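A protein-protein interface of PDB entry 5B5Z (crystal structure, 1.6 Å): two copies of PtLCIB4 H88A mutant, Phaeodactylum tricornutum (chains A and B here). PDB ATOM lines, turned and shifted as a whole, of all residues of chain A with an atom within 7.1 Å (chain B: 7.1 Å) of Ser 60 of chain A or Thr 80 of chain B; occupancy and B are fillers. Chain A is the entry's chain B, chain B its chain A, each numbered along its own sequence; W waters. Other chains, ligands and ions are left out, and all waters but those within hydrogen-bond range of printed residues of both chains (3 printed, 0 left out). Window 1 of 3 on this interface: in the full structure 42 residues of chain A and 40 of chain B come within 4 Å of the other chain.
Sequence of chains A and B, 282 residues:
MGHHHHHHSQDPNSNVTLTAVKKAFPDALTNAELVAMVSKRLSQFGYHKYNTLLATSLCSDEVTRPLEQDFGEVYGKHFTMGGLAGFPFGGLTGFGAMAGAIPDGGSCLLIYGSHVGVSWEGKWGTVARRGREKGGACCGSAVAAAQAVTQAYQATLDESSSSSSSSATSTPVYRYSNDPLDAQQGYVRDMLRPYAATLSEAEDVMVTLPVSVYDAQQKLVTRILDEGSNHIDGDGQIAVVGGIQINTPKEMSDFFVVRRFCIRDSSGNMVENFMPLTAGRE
The backbone carbonyl oxygen of His 78 of chain B lies within hydrogen-bond range of the guanidinium group of Arg 65 of chain A (2.9 Å).
O of Ser 60 of chain A sits at hydrogen-bond distance from N of Thr 80 of chain B (3.0 Å).
The guanidinium group of Arg 65 of chain A is in salt-bridge range of the side-chain carboxylate of Glu 68 of chain A, 2.8 Å away.
The guanidinium group (NH1) of Arg 65 of chain A lies within hydrogen-bond range of the side-chain hydroxyl (OG1) of Thr 64 of chain A (3.0 Å).
The backbone carbonyl oxygen (O) of Ser 60 of chain A is in hydrogen-bond range of the guanidinium group (NH2) of Arg 65 of chain A (3.0 Å).
The backbone carbonyl oxygen (O) of Asp 61 of chain A lies within hydrogen-bond range of the guanidinium group (NH2) of Arg 65 of chain A, 3.2 Å away.
SG of Cys 59 of chain A sits close to N of Asp 61 of chain A, 3.5 Å away.
The side-chain hydroxyl of Thr 64 of chain A sits at hydrogen-bond distance from the backbone carbonyl oxygen of Asp 61 of chain A, at 3.0 Å.
Among the printed residues, pairs that only touch across the chains: Ser 60 of chain A with Phe 79 of chain B, Asp 61 of chain A with Phe 79 of chain B, Glu 62 of chain A with His 78 of chain B, Glu 62 of chain A with Phe 79 of chain B, Arg 65 of chain A with Thr 80 of chain B, Thr 80 of chain A with Arg 65 of chain B, Leu 84 of chain A with Gly 90 of chain B, Leu 84 of chain A with Gly 94 of chain B and Gln 184 of chain A with Gly 90 of chain B.
Of chain B, only Phe 79 (3.6 Å) and Thr 80 (3.0 Å) come within 4 Å of Ser 60 of chain A.
Val 63 of chain A touches none of the printed residues of chain B.
Printed residues of chain B within 4 Å of Gln 184 of chain A: Gly 90 (3.9 Å).
Ala 55 of chain B touches none of the printed residues of chain A.
Of the printed residues of chain A, Phe 79 of chain B touches Ser 60 (3.6 Å), Asp 61 (3.5 Å) and Glu 62 (3.2 Å).
Of the printed residues of chain A, Gly 94 of chain B touches Leu 84 (3.9 Å).
The nearest residue of chain B that does not touch Ser 60 of chain A is His 78 of chain B (4.4 Å).
The nearest residue of chain A that does not touch Thr 80 of chain B is Cys 59 of chain A (5.0 Å).
The nearest printed residue of chain B that does not touch Leu 84 of chain A is Ala 97 of chain B (5.3 Å).
Of the 18 printed residues of chain A, 7 touch a printed residue of chain B.
Hydrophobic or aromatic side chains of chain A that line the printed part of chain B: Leu 84.
Of the 18 printed residues of chain B, 6 touch a printed residue of chain A.
Among the printed residues, 11 pairs touch across the chains.
Among the printed residues, no Asp or Glu carboxylate lies within 4 Å of a Lys or Arg side-chain nitrogen of the other chain.
Arg 65 of chain A touches Thr 80 of chain B, and with the chains exchanged Thr 80 of chain A touches Arg 65 of chain B.
Positions printed for both chains: 58, 65, 68, 80, 82 and 83.
Of the 11 pairs that touch across the chains among the printed residues, 2 have their exchanged pair printed and touching as well.
Water W3 lies within hydrogen-bond range of the backbone carbonyl oxygen of Gly 82 of chain A, the side-chain amide nitrogen of Gln 184 of chain A and the backbone carbonyl oxygen of Gly 82 of chain B.
Water W1 lies within hydrogen-bond range of O of Thr 80 of chain B (3.0 Å), OG of Ser 60 of chain A (3.1 Å) and SD of Met 81 of chain B (3.7 Å).
Water W2 lies within hydrogen-bond range of the backbone carbonyl oxygen of Gly 90 of chain B (3.0 Å) and the backbone NH of Gln 184 of chain A (3.3 Å).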
ATOM      1  N   LEU A  58      27.437 -24.304 -22.606  1.00  0.00           N
ATOM      2  CA  LEU A  58      28.611 -23.851 -23.337  1.00  0.00           C
ATOM      3  C   LEU A  58      28.491 -22.344 -23.569  1.00  0.00           C
ATOM      4  O   LEU A  58      27.409 -21.783 -23.416  1.00  0.00           O
ATOM      5  CB  LEU A  58      28.752 -24.617 -24.653  1.00  0.00           C
ATOM      6  CG  LEU A  58      28.971 -26.136 -24.532  1.00  0.00           C
ATOM      7  CD1 LEU A  58      28.840 -26.784 -25.908  1.00  0.00           C
ATOM      8  CD2 LEU A  58      30.308 -26.482 -23.890  1.00  0.00           C
ATOM      9  N   CYS A  59      29.603 -21.681 -23.882  1.00  0.00           N
ATOM     10  CA  CYS A  59      29.554 -20.228 -24.022  1.00  0.00           C
ATOM     11  C   CYS A  59      28.606 -19.829 -25.165  1.00  0.00           C
ATOM     12  O   CYS A  59      28.478 -20.519 -26.180  1.00  0.00           O
ATOM     13  CB  CYS A  59      30.965 -19.655 -24.247  1.00  0.00           C
ATOM     14  SG  CYS A  59      31.029 -17.828 -24.299  1.00  0.00           S
ATOM     15  N   SER A  60      27.952 -18.689 -24.994  1.00  0.00           N
ATOM     16  CA  SER A  60      27.103 -18.138 -26.025  1.00  0.00           C
ATOM     17  C   SER A  60      27.829 -17.761 -27.319  1.00  0.00           C
ATOM     18  O   SER A  60      27.181 -17.580 -28.333  1.00  0.00           O
ATOM     19  CB  SER A  60      26.385 -16.929 -25.461  1.00  0.00           C
ATOM     20  OG  SER A  60      27.312 -16.166 -24.717  1.00  0.00           O
ATOM     21  N   ASP A  61      29.157 -17.625 -27.278  1.00  0.00           N
ATOM     22  CA  ASP A  61      29.993 -17.331 -28.454  1.00  0.00           C
ATOM     23  C   ASP A  61      29.674 -18.257 -29.642  1.00  0.00           C
ATOM     24  O   ASP A  61      29.511 -19.454 -29.447  1.00  0.00           O
ATOM     25  CB  ASP A  61      31.453 -17.485 -28.017  1.00  0.00           C
ATOM     26  CG  ASP A  61      32.453 -16.884 -28.981  1.00  0.00           C
ATOM     27  OD1 ASP A  61      32.235 -16.927 -30.214  1.00  0.00           O
ATOM     28  OD2 ASP A  61      33.503 -16.416 -28.471  1.00  0.00           O
ATOM     29  N   GLU A  62      29.574 -17.712 -30.855  1.00  0.00           N
ATOM     30  CA  GLU A  62      29.294 -18.551 -32.035  1.00  0.00           C
ATOM     31  C   GLU A  62      30.324 -19.667 -32.243  1.00  0.00           C
ATOM     32  O   GLU A  62      29.997 -20.685 -32.838  1.00  0.00           O
ATOM     33  CB  GLU A  62      29.204 -17.712 -33.331  1.00  0.00           C
ATOM     34  CG  GLU A  62      30.460 -16.901 -33.682  1.00  0.00           C
ATOM     35  CD  GLU A  62      31.502 -17.619 -34.539  1.00  0.00           C
ATOM     36  OE1 GLU A  62      32.447 -16.936 -35.000  1.00  0.00           O
ATOM     37  OE2 GLU A  62      31.398 -18.843 -34.761  1.00  0.00           O
ATOM     38  N   VAL A  63      31.557 -19.494 -31.767  1.00  0.00           N
ATOM     39  CA  VAL A  63      32.581 -20.515 -32.017  1.00  0.00           C
ATOM     40  C   VAL A  63      32.289 -21.823 -31.283  1.00  0.00           C
ATOM     41  O   VAL A  63      32.890 -22.854 -31.586  1.00  0.00           O
ATOM     42  CB  VAL A  63      34.010 -20.045 -31.620  1.00  0.00           C
ATOM     43  CG1 VAL A  63      34.364 -18.755 -32.340  1.00  0.00           C
ATOM     44  CG2 VAL A  63      34.156 -19.921 -30.094  1.00  0.00           C
ATOM     45  N   THR A  64      31.386 -21.804 -30.313  1.00  0.00           N
ATOM     46  CA  THR A  64      31.138 -23.042 -29.599  1.00  0.00           C
ATOM     47  C   THR A  64      30.081 -23.924 -30.285  1.00  0.00           C
ATOM     48  O   THR A  64      29.971 -25.094 -29.949  1.00  0.00           O
ATOM     49  CB  THR A  64      30.733 -22.785 -28.121  1.00  0.00           C
ATOM     50  OG1 THR A  64      29.491 -22.092 -28.084  1.00  0.00           O
ATOM     51  CG2 THR A  64      31.815 -21.975 -27.403  1.00  0.00           C
ATOM     52  N   ARG A  65      29.346 -23.384 -31.270  1.00  0.00           N
ATOM     53  CA  ARG A  65      28.289 -24.132 -31.990  1.00  0.00           C
ATOM     54  C   ARG A  65      28.688 -25.483 -32.635  1.00  0.00           C
ATOM     55  O   ARG A  65      27.865 -26.403 -32.645  1.00  0.00           O
ATOM     56  CB  ARG A  65      27.648 -23.259 -33.097  1.00  0.00           C
ATOM     57  CG  ARG A  65      26.999 -21.913 -32.651  1.00  0.00           C
ATOM     58  CD  ARG A  65      25.702 -22.018 -31.820  1.00  0.00           C
ATOM     59  NE  ARG A  65      25.964 -22.235 -30.396  1.00  0.00           N
ATOM     60  CZ  ARG A  65      26.282 -21.276 -29.529  1.00  0.00           C
ATOM     61  NH1 ARG A  65      26.500 -21.589 -28.256  1.00  0.00           N
ATOM     62  NH2 ARG A  65      26.381 -20.010 -29.926  1.00  0.00           N
ATOM     63  N   GLU A  68      28.031 -28.425 -30.343  1.00  0.00           N
ATOM     64  CA  GLU A  68      26.613 -28.692 -30.198  1.00  0.00           C
ATOM     65  C   GLU A  68      26.072 -29.393 -31.433  1.00  0.00           C
ATOM     66  O   GLU A  68      25.270 -30.324 -31.318  1.00  0.00           O
ATOM     67  CB  GLU A  68      25.830 -27.395 -29.942  1.00  0.00           C
ATOM     68  CG  GLU A  68      26.227 -26.701 -28.658  1.00  0.00           C
ATOM     69  CD  GLU A  68      25.434 -25.442 -28.395  1.00  0.00           C
ATOM     70  OE1 GLU A  68      25.130 -24.724 -29.374  1.00  0.00           O
ATOM     71  OE2 GLU A  68      25.127 -25.182 -27.208  1.00  0.00           O
ATOM     72  N   THR A  80      19.520 -25.736 -24.012  1.00  0.00           N
ATOM     73  CA  THR A  80      20.720 -24.990 -23.638  1.00  0.00           C
ATOM     74  C   THR A  80      20.599 -24.494 -22.202  1.00  0.00           C
ATOM     75  O   THR A  80      19.543 -24.070 -21.763  1.00  0.00           O
ATOM     76  CB  THR A  80      20.994 -23.821 -24.594  1.00  0.00           C
ATOM     77  OG1 THR A  80      19.955 -22.860 -24.490  1.00  0.00           O
ATOM     78  CG2 THR A  80      21.035 -24.291 -26.041  1.00  0.00           C
ATOM     79  N   GLY A  82      23.501 -22.817 -20.878  1.00  0.00           N
ATOM     80  CA  GLY A  82      24.695 -21.991 -20.746  1.00  0.00           C
ATOM     81  C   GLY A  82      24.444 -20.498 -20.849  1.00  0.00           C
ATOM     82  O   GLY A  82      23.329 -20.009 -20.655  1.00  0.00           O
ATOM     83  N   GLY A  83      25.507 -19.768 -21.136  1.00  0.00           N
ATOM     84  CA  GLY A  83      25.473 -18.322 -21.199  1.00  0.00           C
ATOM     85  C   GLY A  83      26.932 -17.902 -21.286  1.00  0.00           C
ATOM     86  O   GLY A  83      27.766 -18.698 -21.691  1.00  0.00           O
ATOM     87  N   LEU A  84      27.241 -16.668 -20.895  1.00  0.00           N
ATOM     88  CA  LEU A  84      28.621 -16.177 -20.993  1.00  0.00           C
ATOM     89  C   LEU A  84      29.622 -17.092 -20.280  1.00  0.00           C
ATOM     90  O   LEU A  84      29.403 -17.491 -19.119  1.00  0.00           O
ATOM     91  CB  LEU A  84      28.708 -14.761 -20.415  1.00  0.00           C
ATOM     92  CG  LEU A  84      27.941 -13.658 -21.143  1.00  0.00           C
ATOM     93  CD1 LEU A  84      28.212 -12.340 -20.410  1.00  0.00           C
ATOM     94  CD2 LEU A  84      28.381 -13.554 -22.583  1.00  0.00           C
ATOM     95  N   ALA A  85      30.691 -17.435 -21.012  1.00  0.00           N
ATOM     96  CA  ALA A  85      31.810 -18.254 -20.535  1.00  0.00           C
ATOM     97  C   ALA A  85      31.447 -19.719 -20.304  1.00  0.00           C
ATOM     98  O   ALA A  85      32.315 -20.497 -19.935  1.00  0.00           O
ATOM     99  CB  ALA A  85      32.416 -17.659 -19.243  1.00  0.00           C
ATOM    100  N   GLY A  86      30.189 -20.083 -20.579  1.00  0.00           N
ATOM    101  CA  GLY A  86      29.720 -21.454 -20.452  1.00  0.00           C
ATOM    102  C   GLY A  86      29.093 -21.831 -19.114  1.00  0.00           C
ATOM    103  O   GLY A  86      28.727 -22.986 -18.915  1.00  0.00           O
ATOM    104  N   HIS A 115      35.765 -22.578 -22.749  1.00  0.00           N
ATOM    105  CA  HIS A 115      36.413 -22.700 -24.031  1.00  0.00           C
ATOM    106  C   HIS A 115      37.552 -21.692 -24.158  1.00  0.00           C
ATOM    107  O   HIS A 115      37.648 -20.732 -23.384  1.00  0.00           O
ATOM    108  CB  HIS A 115      35.401 -22.557 -25.174  1.00  0.00           C
ATOM    109  CG  HIS A 115      34.989 -21.149 -25.472  1.00  0.00           C
ATOM    110  ND1 HIS A 115      35.225 -20.596 -26.711  1.00  0.00           N
ATOM    111  CD2 HIS A 115      34.334 -20.200 -24.755  1.00  0.00           C
ATOM    112  CE1 HIS A 115      34.755 -19.371 -26.747  1.00  0.00           C
ATOM    113  NE2 HIS A 115      34.240 -19.096 -25.564  1.00  0.00           N
ATOM    114  N   SER A 141      34.398 -13.262 -22.698  1.00  0.00           N
ATOM    115  CA  SER A 141      33.830 -13.045 -21.383  1.00  0.00           C
ATOM    116  C   SER A 141      34.793 -13.424 -20.274  1.00  0.00           C
ATOM    117  O   SER A 141      34.945 -12.682 -19.302  1.00  0.00           O
ATOM    118  CB  SER A 141      32.525 -13.839 -21.237  1.00  0.00           C
ATOM    119  OG  SER A 141      32.190 -14.009 -19.875  1.00  0.00           O
ATOM    120  N   GLN A 184      24.914 -11.331 -16.085  1.00  0.00           N
ATOM    121  CA  GLN A 184      25.730 -12.520 -16.348  1.00  0.00           C
ATOM    122  C   GLN A 184      27.220 -12.261 -16.216  1.00  0.00           C
ATOM    123  O   GLN A 184      27.943 -13.033 -15.579  1.00  0.00           O
ATOM    124  CB  GLN A 184      25.425 -13.092 -17.743  1.00  0.00           C
ATOM    125  CG  GLN A 184      24.652 -14.376 -17.639  1.00  0.00           C
ATOM    126  CD  GLN A 184      24.255 -14.998 -18.959  1.00  0.00           C
ATOM    127  OE1 GLN A 184      25.020 -15.024 -19.937  1.00  0.00           O
ATOM    128  NE2 GLN A 184      23.052 -15.558 -18.977  1.00  0.00           N
ATOM    129  N   LEU B  54      24.772 -13.783 -37.458  1.00  0.00           N
ATOM    130  CA  LEU B  54      23.460 -14.119 -36.917  1.00  0.00           C
ATOM    131  C   LEU B  54      23.517 -14.199 -35.393  1.00  0.00           C
ATOM    132  O   LEU B  54      24.459 -14.767 -34.827  1.00  0.00           O
ATOM    133  CB  LEU B  54      22.986 -15.441 -37.507  1.00  0.00           C
ATOM    134  CG  LEU B  54      21.640 -15.963 -37.013  1.00  0.00           C
ATOM    135  CD1 LEU B  54      20.518 -15.008 -37.390  1.00  0.00           C
ATOM    136  CD2 LEU B  54      21.384 -17.365 -37.557  1.00  0.00           C
ATOM    137  N   ALA B  55      22.528 -13.604 -34.725  1.00  0.00           N
ATOM    138  CA  ALA B  55      22.405 -13.759 -33.270  1.00  0.00           C
ATOM    139  C   ALA B  55      20.964 -14.066 -32.928  1.00  0.00           C
ATOM    140  O   ALA B  55      20.062 -13.604 -33.609  1.00  0.00           O
ATOM    141  CB  ALA B  55      22.878 -12.498 -32.540  1.00  0.00           C
ATOM    142  N   THR B  56      20.752 -14.850 -31.876  1.00  0.00           N
ATOM    143  CA  THR B  56      19.382 -15.140 -31.429  1.00  0.00           C
ATOM    144  C   THR B  56      19.212 -14.847 -29.937  1.00  0.00           C
ATOM    145  O   THR B  56      20.165 -14.931 -29.156  1.00  0.00           O
ATOM    146  CB  THR B  56      18.980 -16.605 -31.681  1.00  0.00           C
ATOM    147  OG1 THR B  56      19.716 -17.471 -30.810  1.00  0.00           O
ATOM    148  CG2 THR B  56      19.219 -17.025 -33.144  1.00  0.00           C
ATOM    149  N   SER B  57      17.986 -14.495 -29.567  1.00  0.00           N
ATOM    150  CA  SER B  57      17.574 -14.454 -28.170  1.00  0.00           C
ATOM    151  C   SER B  57      16.237 -15.188 -28.093  1.00  0.00           C
ATOM    152  O   SER B  57      15.156 -14.605 -28.274  1.00  0.00           O
ATOM    153  CB  SER B  57      17.461 -13.016 -27.654  1.00  0.00           C
ATOM    154  OG  SER B  57      17.218 -13.007 -26.244  1.00  0.00           O
ATOM    155  N   LEU B  58      16.348 -16.490 -27.897  1.00  0.00           N
ATOM    156  CA  LEU B  58      15.202 -17.393 -27.851  1.00  0.00           C
ATOM    157  C   LEU B  58      15.297 -18.253 -26.599  1.00  0.00           C
ATOM    158  O   LEU B  58      16.367 -18.339 -25.980  1.00  0.00           O
ATOM    159  CB  LEU B  58      15.162 -18.272 -29.107  1.00  0.00           C
ATOM    160  CG  LEU B  58      15.089 -17.510 -30.442  1.00  0.00           C
ATOM    161  CD1 LEU B  58      15.354 -18.436 -31.657  1.00  0.00           C
ATOM    162  CD2 LEU B  58      13.743 -16.796 -30.585  1.00  0.00           C
ATOM    163  N   ARG B  65      14.910 -24.707 -31.096  1.00  0.00           N
ATOM    164  CA  ARG B  65      16.037 -24.935 -32.005  1.00  0.00           C
ATOM    165  C   ARG B  65      15.728 -24.896 -33.517  1.00  0.00           C
ATOM    166  O   ARG B  65      16.572 -24.428 -34.280  1.00  0.00           O
ATOM    167  CB  ARG B  65      16.722 -26.278 -31.689  1.00  0.00           C
ATOM    168  CG  ARG B  65      17.302 -26.434 -30.253  1.00  0.00           C
ATOM    169  CD  ARG B  65      18.536 -25.591 -29.958  1.00  0.00           C
ATOM    170  NE  ARG B  65      18.177 -24.246 -29.520  1.00  0.00           N
ATOM    171  CZ  ARG B  65      17.808 -23.942 -28.278  1.00  0.00           C
ATOM    172  NH1 ARG B  65      17.486 -22.688 -27.976  1.00  0.00           N
ATOM    173  NH2 ARG B  65      17.760 -24.887 -27.337  1.00  0.00           N
ATOM    174  N   GLU B  68      16.386 -21.456 -35.077  1.00  0.00           N
ATOM    175  CA  GLU B  68      17.809 -21.157 -35.164  1.00  0.00           C
ATOM    176  C   GLU B  68      18.456 -21.901 -36.319  1.00  0.00           C
ATOM    177  O   GLU B  68      19.288 -21.334 -37.032  1.00  0.00           O
ATOM    178  CB  GLU B  68      18.521 -21.517 -33.858  1.00  0.00           C
ATOM    179  CG  GLU B  68      17.960 -20.780 -32.664  1.00  0.00           C
ATOM    180  CD  GLU B  68      18.737 -21.062 -31.396  1.00  0.00           C
ATOM    181  OE1 GLU B  68      19.222 -22.210 -31.251  1.00  0.00           O
ATOM    182  OE2 GLU B  68      18.886 -20.127 -30.571  1.00  0.00           O
ATOM    183  N   HIS B  78      25.554 -19.066 -35.165  1.00  0.00           N
ATOM    184  CA  HIS B  78      25.021 -17.894 -34.483  1.00  0.00           C
ATOM    185  C   HIS B  78      25.551 -17.713 -33.069  1.00  0.00           C
ATOM    186  O   HIS B  78      25.925 -18.682 -32.409  1.00  0.00           O
ATOM    187  CB  HIS B  78      23.503 -17.989 -34.407  1.00  0.00           C
ATOM    188  CG  HIS B  78      23.024 -19.134 -33.570  1.00  0.00           C
ATOM    189  ND1 HIS B  78      23.027 -20.434 -34.024  1.00  0.00           N
ATOM    190  CD2 HIS B  78      22.510 -19.175 -32.318  1.00  0.00           C
ATOM    191  CE1 HIS B  78      22.554 -21.230 -33.080  1.00  0.00           C
ATOM    192  NE2 HIS B  78      22.233 -20.492 -32.034  1.00  0.00           N
ATOM    193  N   PHE B  79      25.558 -16.461 -32.626  1.00  0.00           N
ATOM    194  CA  PHE B  79      25.725 -16.109 -31.220  1.00  0.00           C
ATOM    195  C   PHE B  79      24.411 -16.302 -30.496  1.00  0.00           C
ATOM    196  O   PHE B  79      23.366 -15.974 -31.034  1.00  0.00           O
ATOM    197  CB  PHE B  79      26.160 -14.643 -31.071  1.00  0.00           C
ATOM    198  CG  PHE B  79      27.642 -14.437 -30.983  1.00  0.00           C
ATOM    199  CD1 PHE B  79      28.420 -14.439 -32.128  1.00  0.00           C
ATOM    200  CD2 PHE B  79      28.255 -14.196 -29.752  1.00  0.00           C
ATOM    201  CE1 PHE B  79      29.803 -14.219 -32.052  1.00  0.00           C
ATOM    202  CE2 PHE B  79      29.631 -13.995 -29.677  1.00  0.00           C
ATOM    203  CZ  PHE B  79      30.400 -14.002 -30.828  1.00  0.00           C
ATOM    204  N   THR B  80      24.437 -16.799 -29.273  1.00  0.00           N
ATOM    205  CA  THR B  80      23.198 -16.804 -28.500  1.00  0.00           C
ATOM    206  C   THR B  80      23.207 -15.717 -27.431  1.00  0.00           C
ATOM    207  O   THR B  80      24.235 -15.388 -26.828  1.00  0.00           O
ATOM    208  CB  THR B  80      22.941 -18.168 -27.877  1.00  0.00           C
ATOM    209  OG1 THR B  80      24.032 -18.518 -27.038  1.00  0.00           O
ATOM    210  CG2 THR B  80      22.811 -19.215 -28.962  1.00  0.00           C
ATOM    211  N   MET B  81      22.053 -15.102 -27.250  1.00  0.00           N
ATOM    212  CA  MET B  81      21.896 -14.064 -26.261  1.00  0.00           C
ATOM    213  C   MET B  81      20.834 -14.454 -25.246  1.00  0.00           C
ATOM    214  O   MET B  81      20.641 -13.762 -24.257  1.00  0.00           O
ATOM    215  CB  MET B  81      21.495 -12.746 -26.930  1.00  0.00           C
ATOM    216  CG  MET B  81      22.620 -12.040 -27.649  1.00  0.00           C
ATOM    217  SD  MET B  81      23.557 -11.034 -26.469  1.00  0.00           S
ATOM    218  CE  MET B  81      22.335  -9.828 -25.887  1.00  0.00           C
ATOM    219  N   GLY B  82      20.126 -15.543 -25.525  1.00  0.00           N
ATOM    220  CA  GLY B  82      18.896 -15.862 -24.798  1.00  0.00           C
ATOM    221  C   GLY B  82      19.115 -16.595 -23.481  1.00  0.00           C
ATOM    222  O   GLY B  82      20.195 -16.571 -22.882  1.00  0.00           O
ATOM    223  N   GLY B  83      18.057 -17.245 -23.019  1.00  0.00           N
ATOM    224  CA  GLY B  83      18.045 -17.883 -21.713  1.00  0.00           C
ATOM    225  C   GLY B  83      16.597 -18.224 -21.464  1.00  0.00           C
ATOM    226  O   GLY B  83      15.833 -18.262 -22.406  1.00  0.00           O
ATOM    227  N   GLY B  90      22.241 -12.518 -22.020  1.00  0.00           N
ATOM    228  CA  GLY B  90      23.631 -12.211 -22.330  1.00  0.00           C
ATOM    229  C   GLY B  90      23.938 -10.750 -22.035  1.00  0.00           C
ATOM    230  O   GLY B  90      25.076 -10.392 -21.732  1.00  0.00           O
ATOM    231  N   GLY B  94      27.215  -9.632 -23.547  1.00  0.00           N
ATOM    232  CA  GLY B  94      26.869 -10.534 -24.624  1.00  0.00           C
ATOM    233  C   GLY B  94      26.700  -9.795 -25.940  1.00  0.00           C
ATOM    234  O   GLY B  94      27.164 -10.258 -26.989  1.00  0.00           O
ATOM    235  N   PHE B  95      26.041  -8.641 -25.903  1.00  0.00           N
ATOM    236  CA  PHE B  95      25.880  -7.860 -27.120  1.00  0.00           C
ATOM    237  C   PHE B  95      27.225  -7.363 -27.639  1.00  0.00           C
ATOM    238  O   PHE B  95      27.496  -7.402 -28.842  1.00  0.00           O
ATOM    239  CB  PHE B  95      24.956  -6.666 -26.882  1.00  0.00           C
ATOM    240  CG  PHE B  95      24.688  -5.867 -28.122  1.00  0.00           C
ATOM    241  CD1 PHE B  95      23.783  -6.321 -29.064  1.00  0.00           C
ATOM    242  CD2 PHE B  95      25.368  -4.683 -28.366  1.00  0.00           C
ATOM    243  CE1 PHE B  95      23.552  -5.603 -30.218  1.00  0.00           C
ATOM    244  CE2 PHE B  95      25.132  -3.963 -29.521  1.00  0.00           C
ATOM    245  CZ  PHE B  95      24.227  -4.424 -30.443  1.00  0.00           C
ATOM    246  N   ALA B  97      30.110  -8.750 -27.145  1.00  0.00           N
ATOM    247  CA  ALA B  97      30.837  -9.909 -27.650  1.00  0.00           C
ATOM    248  C   ALA B  97      30.422 -10.215 -29.081  1.00  0.00           C
ATOM    249  O   ALA B  97      31.242 -10.488 -29.959  1.00  0.00           O
ATOM    250  CB  ALA B  97      30.584 -11.115 -26.757  1.00  0.00           C
ATOM    251  N   MET B  98      29.122 -10.172 -29.304  1.00  0.00           N
ATOM    252  CA  MET B  98      28.579 -10.399 -30.621  1.00  0.00           C
ATOM    253  C   MET B  98      29.088  -9.325 -31.597  1.00  0.00           C
ATOM    254  O   MET B  98      29.555  -9.646 -32.689  1.00  0.00           O
ATOM    255  CB  MET B  98      27.044 -10.422 -30.526  1.00  0.00           C
ATOM    256  CG  MET B  98      26.342 -10.799 -31.791  1.00  0.00           C
ATOM    257  SD  MET B  98      26.267  -9.365 -32.868  1.00  0.00           S
ATOM    258  CE  MET B  98      25.308  -8.220 -31.870  1.00  0.00           C
HETATM  259  O   HOH W   1      25.480 -13.715 -24.696  1.00  0.00           O
HETATM  260  O   HOH W   2      25.896  -9.923 -18.892  1.00  0.00           O
HETATM  261  O   HOH W   3      21.728 -17.593 -20.608  1.00  0.00           O
